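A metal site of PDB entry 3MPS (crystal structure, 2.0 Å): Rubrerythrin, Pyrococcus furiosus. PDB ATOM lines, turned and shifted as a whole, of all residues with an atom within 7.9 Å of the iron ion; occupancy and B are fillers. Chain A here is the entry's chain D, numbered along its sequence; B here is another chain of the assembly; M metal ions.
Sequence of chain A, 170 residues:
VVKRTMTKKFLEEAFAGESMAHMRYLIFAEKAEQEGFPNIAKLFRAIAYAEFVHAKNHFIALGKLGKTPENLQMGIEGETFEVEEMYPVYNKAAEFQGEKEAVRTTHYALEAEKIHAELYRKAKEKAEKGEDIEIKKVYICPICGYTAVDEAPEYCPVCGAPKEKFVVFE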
ATOM      1  N   TYR A 108      23.902  27.168  33.360  1.00  0.00           N
ATOM      2  CA  TYR A 108      23.221  26.387  32.291  1.00  0.00           C
ATOM      3  C   TYR A 108      24.110  25.267  31.755  1.00  0.00           C
ATOM      4  O   TYR A 108      23.729  24.082  31.786  1.00  0.00           O
ATOM      5  CB  TYR A 108      22.792  27.291  31.120  1.00  0.00           C
ATOM      6  CG  TYR A 108      21.580  28.151  31.369  1.00  0.00           C
ATOM      7  CD1 TYR A 108      20.708  27.883  32.425  1.00  0.00           C
ATOM      8  CD2 TYR A 108      21.293  29.220  30.540  1.00  0.00           C
ATOM      9  CE1 TYR A 108      19.590  28.676  32.645  1.00  0.00           C
ATOM     10  CE2 TYR A 108      20.157  30.015  30.742  1.00  0.00           C
ATOM     11  CZ  TYR A 108      19.321  29.729  31.811  1.00  0.00           C
ATOM     12  OH  TYR A 108      18.211  30.483  32.044  1.00  0.00           O
ATOM     13  N   ALA A 112      23.737  21.278  31.995  1.00  0.00           N
ATOM     14  CA  ALA A 112      23.328  20.720  30.706  1.00  0.00           C
ATOM     15  C   ALA A 112      24.414  19.862  30.040  1.00  0.00           C
ATOM     16  O   ALA A 112      24.105  18.994  29.225  1.00  0.00           O
ATOM     17  CB  ALA A 112      22.873  21.840  29.768  1.00  0.00           C
ATOM     18  N   ILE A 140      17.198  19.251  22.126  1.00  0.00           N
ATOM     19  CA  ILE A 140      18.067  20.237  22.748  1.00  0.00           C
ATOM     20  C   ILE A 140      17.283  21.503  23.039  1.00  0.00           C
ATOM     21  O   ILE A 140      16.563  22.007  22.182  1.00  0.00           O
ATOM     22  CB  ILE A 140      19.325  20.555  21.902  1.00  0.00           C
ATOM     23  CG1 ILE A 140      20.169  19.285  21.689  1.00  0.00           C
ATOM     24  CG2 ILE A 140      20.219  21.546  22.599  1.00  0.00           C
ATOM     25  CD1 ILE A 140      19.932  18.678  20.414  1.00  0.00           C
ATOM     26  N   CYS A 141      17.401  21.973  24.284  1.00  0.00           N
ATOM     27  CA  CYS A 141      16.757  23.200  24.684  1.00  0.00           C
ATOM     28  C   CYS A 141      17.511  24.407  24.113  1.00  0.00           C
ATOM     29  O   CYS A 141      18.712  24.555  24.361  1.00  0.00           O
ATOM     30  CB  CYS A 141      16.719  23.289  26.201  1.00  0.00           C
ATOM     31  SG  CYS A 141      16.059  24.859  26.809  1.00  0.00           S
ATOM     32  N   PRO A 142      16.806  25.286  23.359  1.00  0.00           N
ATOM     33  CA  PRO A 142      17.429  26.455  22.723  1.00  0.00           C
ATOM     34  C   PRO A 142      17.851  27.548  23.730  1.00  0.00           C
ATOM     35  O   PRO A 142      18.596  28.476  23.342  1.00  0.00           O
ATOM     36  CB  PRO A 142      16.322  26.988  21.810  1.00  0.00           C
ATOM     37  CG  PRO A 142      15.050  26.576  22.496  1.00  0.00           C
ATOM     38  CD  PRO A 142      15.365  25.216  23.071  1.00  0.00           C
ATOM     39  N   ILE A 143      17.399  27.446  24.979  1.00  0.00           N
ATOM     40  CA  ILE A 143      17.723  28.426  26.019  1.00  0.00           C
ATOM     41  C   ILE A 143      19.041  28.111  26.753  1.00  0.00           C
ATOM     42  O   ILE A 143      19.899  28.981  26.894  1.00  0.00           O
ATOM     43  CB  ILE A 143      16.577  28.564  27.051  1.00  0.00           C
ATOM     44  CG1 ILE A 143      15.302  29.045  26.370  1.00  0.00           C
ATOM     45  CG2 ILE A 143      16.953  29.568  28.165  1.00  0.00           C
ATOM     46  CD1 ILE A 143      14.230  29.527  27.333  1.00  0.00           C
ATOM     47  N   CYS A 144      19.181  26.860  27.185  1.00  0.00           N
ATOM     48  CA  CYS A 144      20.221  26.455  28.119  1.00  0.00           C
ATOM     49  C   CYS A 144      21.033  25.254  27.646  1.00  0.00           C
ATOM     50  O   CYS A 144      21.988  24.848  28.319  1.00  0.00           O
ATOM     51  CB  CYS A 144      19.574  26.121  29.467  1.00  0.00           C
ATOM     52  SG  CYS A 144      18.633  24.563  29.469  1.00  0.00           S
ATOM     53  N   GLY A 145      20.649  24.668  26.518  1.00  0.00           N
ATOM     54  CA  GLY A 145      21.381  23.544  25.919  1.00  0.00           C
ATOM     55  C   GLY A 145      21.084  22.180  26.518  1.00  0.00           C
ATOM     56  O   GLY A 145      21.779  21.189  26.198  1.00  0.00           O
ATOM     57  N   TYR A 146      20.057  22.105  27.365  1.00  0.00           N
ATOM     58  CA  TYR A 146      19.670  20.843  28.006  1.00  0.00           C
ATOM     59  C   TYR A 146      19.397  19.782  26.942  1.00  0.00           C
ATOM     60  O   TYR A 146      18.656  20.016  25.984  1.00  0.00           O
ATOM     61  CB  TYR A 146      18.482  21.033  28.958  1.00  0.00           C
ATOM     62  CG  TYR A 146      18.204  19.831  29.838  1.00  0.00           C
ATOM     63  CD1 TYR A 146      18.836  19.684  31.068  1.00  0.00           C
ATOM     64  CD2 TYR A 146      17.292  18.845  29.458  1.00  0.00           C
ATOM     65  CE1 TYR A 146      18.586  18.600  31.887  1.00  0.00           C
ATOM     66  CE2 TYR A 146      17.043  17.739  30.266  1.00  0.00           C
ATOM     67  CZ  TYR A 146      17.700  17.631  31.484  1.00  0.00           C
ATOM     68  OH  TYR A 146      17.471  16.554  32.301  1.00  0.00           O
ATOM     69  N   THR A 147      20.002  18.624  27.131  1.00  0.00           N
ATOM     70  CA  THR A 147      20.067  17.591  26.106  1.00  0.00           C
ATOM     71  C   THR A 147      19.373  16.322  26.613  1.00  0.00           C
ATOM     72  O   THR A 147      19.710  15.821  27.683  1.00  0.00           O
ATOM     73  CB  THR A 147      21.530  17.286  25.757  1.00  0.00           C
ATOM     74  OG1 THR A 147      22.112  18.470  25.181  1.00  0.00           O
ATOM     75  CG2 THR A 147      21.641  16.111  24.746  1.00  0.00           C
ATOM     76  N   TYR A 155       9.015  19.752  31.104  1.00  0.00           N
ATOM     77  CA  TYR A 155       9.677  21.051  31.091  1.00  0.00           C
ATOM     78  C   TYR A 155      11.178  20.864  31.266  1.00  0.00           C
ATOM     79  O   TYR A 155      11.628  19.836  31.774  1.00  0.00           O
ATOM     80  CB  TYR A 155       9.102  21.998  32.157  1.00  0.00           C
ATOM     81  CG  TYR A 155       9.409  21.599  33.595  1.00  0.00           C
ATOM     82  CD1 TYR A 155      10.567  22.057  34.232  1.00  0.00           C
ATOM     83  CD2 TYR A 155       8.537  20.792  34.324  1.00  0.00           C
ATOM     84  CE1 TYR A 155      10.863  21.715  35.538  1.00  0.00           C
ATOM     85  CE2 TYR A 155       8.826  20.449  35.647  1.00  0.00           C
ATOM     86  CZ  TYR A 155       9.986  20.914  36.243  1.00  0.00           C
ATOM     87  OH  TYR A 155      10.286  20.572  37.539  1.00  0.00           O
ATOM     88  N   CYS A 156      11.952  21.848  30.816  1.00  0.00           N
ATOM     89  CA  CYS A 156      13.392  21.859  31.048  1.00  0.00           C
ATOM     90  C   CYS A 156      13.696  22.035  32.543  1.00  0.00           C
ATOM     91  O   CYS A 156      13.269  23.025  33.153  1.00  0.00           O
ATOM     92  CB  CYS A 156      14.060  22.960  30.224  1.00  0.00           C
ATOM     93  SG  CYS A 156      15.854  22.941  30.285  1.00  0.00           S
ATOM     94  N   PRO A 157      14.425  21.074  33.143  1.00  0.00           N
ATOM     95  CA  PRO A 157      14.800  21.148  34.555  1.00  0.00           C
ATOM     96  C   PRO A 157      15.742  22.316  34.867  1.00  0.00           C
ATOM     97  O   PRO A 157      15.810  22.760  36.005  1.00  0.00           O
ATOM     98  CB  PRO A 157      15.524  19.825  34.821  1.00  0.00           C
ATOM     99  CG  PRO A 157      15.129  18.916  33.669  1.00  0.00           C
ATOM    100  CD  PRO A 157      14.926  19.841  32.513  1.00  0.00           C
ATOM    101  N   VAL A 158      16.457  22.780  33.851  1.00  0.00           N
ATOM    102  CA  VAL A 158      17.470  23.807  34.004  1.00  0.00           C
ATOM    103  C   VAL A 158      16.867  25.211  33.843  1.00  0.00           C
ATOM    104  O   VAL A 158      17.101  26.068  34.682  1.00  0.00           O
ATOM    105  CB  VAL A 158      18.656  23.570  33.017  1.00  0.00           C
ATOM    106  CG1 VAL A 158      19.706  24.680  33.144  1.00  0.00           C
ATOM    107  CG2 VAL A 158      19.298  22.211  33.292  1.00  0.00           C
ATOM    108  N   CYS A 159      16.118  25.454  32.785  1.00  0.00           N
ATOM    109  CA  CYS A 159      15.611  26.805  32.521  1.00  0.00           C
ATOM    110  C   CYS A 159      14.086  27.016  32.660  1.00  0.00           C
ATOM    111  O   CYS A 159      13.632  28.166  32.639  1.00  0.00           O
ATOM    112  CB  CYS A 159      16.101  27.309  31.158  1.00  0.00           C
ATOM    113  SG  CYS A 159      15.205  26.680  29.672  1.00  0.00           S
ATOM    114  N   GLY A 160      13.300  25.944  32.802  1.00  0.00           N
ATOM    115  CA  GLY A 160      11.825  26.061  32.904  1.00  0.00           C
ATOM    116  C   GLY A 160      11.015  25.986  31.608  1.00  0.00           C
ATOM    117  O   GLY A 160       9.803  25.715  31.633  1.00  0.00           O
ATOM    118  N   ALA A 161      11.688  26.202  30.471  1.00  0.00           N
ATOM    119  CA  ALA A 161      11.038  26.101  29.142  1.00  0.00           C
ATOM    120  C   ALA A 161      10.151  24.858  28.958  1.00  0.00           C
ATOM    121  O   ALA A 161      10.559  23.748  29.307  1.00  0.00           O
ATOM    122  CB  ALA A 161      12.103  26.150  28.029  1.00  0.00           C
ATOM    123  N   PRO A 162       8.918  25.042  28.437  1.00  0.00           N
ATOM    124  CA  PRO A 162       8.045  23.907  28.122  1.00  0.00           C
ATOM    125  C   PRO A 162       8.629  22.905  27.112  1.00  0.00           C
ATOM    126  O   PRO A 162       9.486  23.265  26.290  1.00  0.00           O
ATOM    127  CB  PRO A 162       6.775  24.560  27.556  1.00  0.00           C
ATOM    128  CG  PRO A 162       7.156  25.967  27.218  1.00  0.00           C
ATOM    129  CD  PRO A 162       8.271  26.335  28.149  1.00  0.00           C
ATOM    130  N   LYS A 165       9.338  23.804  23.336  1.00  0.00           N
ATOM    131  CA  LYS A 165      10.375  24.736  22.903  1.00  0.00           C
ATOM    132  C   LYS A 165      11.635  23.986  22.439  1.00  0.00           C
ATOM    133  O   LYS A 165      12.435  24.536  21.697  1.00  0.00           O
ATOM    134  CB  LYS A 165      10.726  25.712  24.018  1.00  0.00           C
ATOM    135  CG  LYS A 165       9.525  26.528  24.529  1.00  0.00           C
ATOM    136  CD  LYS A 165       9.380  27.852  23.795  1.00  0.00           C
ATOM    137  CE  LYS A 165       8.066  28.551  24.129  1.00  0.00           C
ATOM    138  NZ  LYS A 165       6.916  27.909  23.414  1.00  0.00           N
ATOM    139  N   PHE A 166      11.775  22.735  22.871  1.00  0.00           N
ATOM    140  CA  PHE A 166      12.949  21.929  22.555  1.00  0.00           C
ATOM    141  C   PHE A 166      13.113  21.743  21.042  1.00  0.00           C
ATOM    142  O   PHE A 166      12.131  21.482  20.330  1.00  0.00           O
ATOM    143  CB  PHE A 166      12.845  20.562  23.241  1.00  0.00           C
ATOM    144  CG  PHE A 166      13.299  20.570  24.684  1.00  0.00           C
ATOM    145  CD1 PHE A 166      14.524  20.029  25.041  1.00  0.00           C
ATOM    146  CD2 PHE A 166      12.482  21.095  25.685  1.00  0.00           C
ATOM    147  CE1 PHE A 166      14.952  20.029  26.387  1.00  0.00           C
ATOM    148  CE2 PHE A 166      12.901  21.092  27.028  1.00  0.00           C
ATOM    149  CZ  PHE A 166      14.129  20.551  27.375  1.00  0.00           C
ATOM    150  N   VAL B  53      24.397  26.896  21.548  1.00  0.00           N
ATOM    151  CA  VAL B  53      23.629  27.588  22.585  1.00  0.00           C
ATOM    152  C   VAL B  53      24.540  28.140  23.686  1.00  0.00           C
ATOM    153  O   VAL B  53      24.418  29.301  24.067  1.00  0.00           O
ATOM    154  CB  VAL B  53      22.511  26.699  23.180  1.00  0.00           C
ATOM    155  CG1 VAL B  53      21.743  27.453  24.304  1.00  0.00           C
ATOM    156  CG2 VAL B  53      21.536  26.263  22.078  1.00  0.00           C
HETATM  157 FE    FE M   1      16.386  24.815  29.082  1.00  0.00          FE
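The nearest printed residue that does not touch the iron ion is Ile 143 (4.3 Å).
The backbone NH (N) of Cys 141 lies within hydrogen-bond range of the backbone carbonyl oxygen (O) of Tyr 146. N of Cys 156 lies within hydrogen-bond range of O of Ala 161 (2.8 Å). The side-chain sulfur (SG) of Cys 144 sits close to the backbone NH (N) of Tyr 146. The backbone NH (N) of Ala 161 sits close to the side-chain sulfur (SG) of Cys 159 (3.6 Å). The backbone NH of Ile 143 lies close to the side-chain sulfur of Cys 141 (3.4 Å). SG of Cys 156 lies close to N of Val 158 (3.6 Å).
The iron ion is bound by SG of Cys 159 (2.3 Å), SG of Cys 156 (2.3 Å), SG of Cys 144 (2.3 Å) and SG of Cys 141 (2.3 Å). The iron ion has four donor atoms within binding distance.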
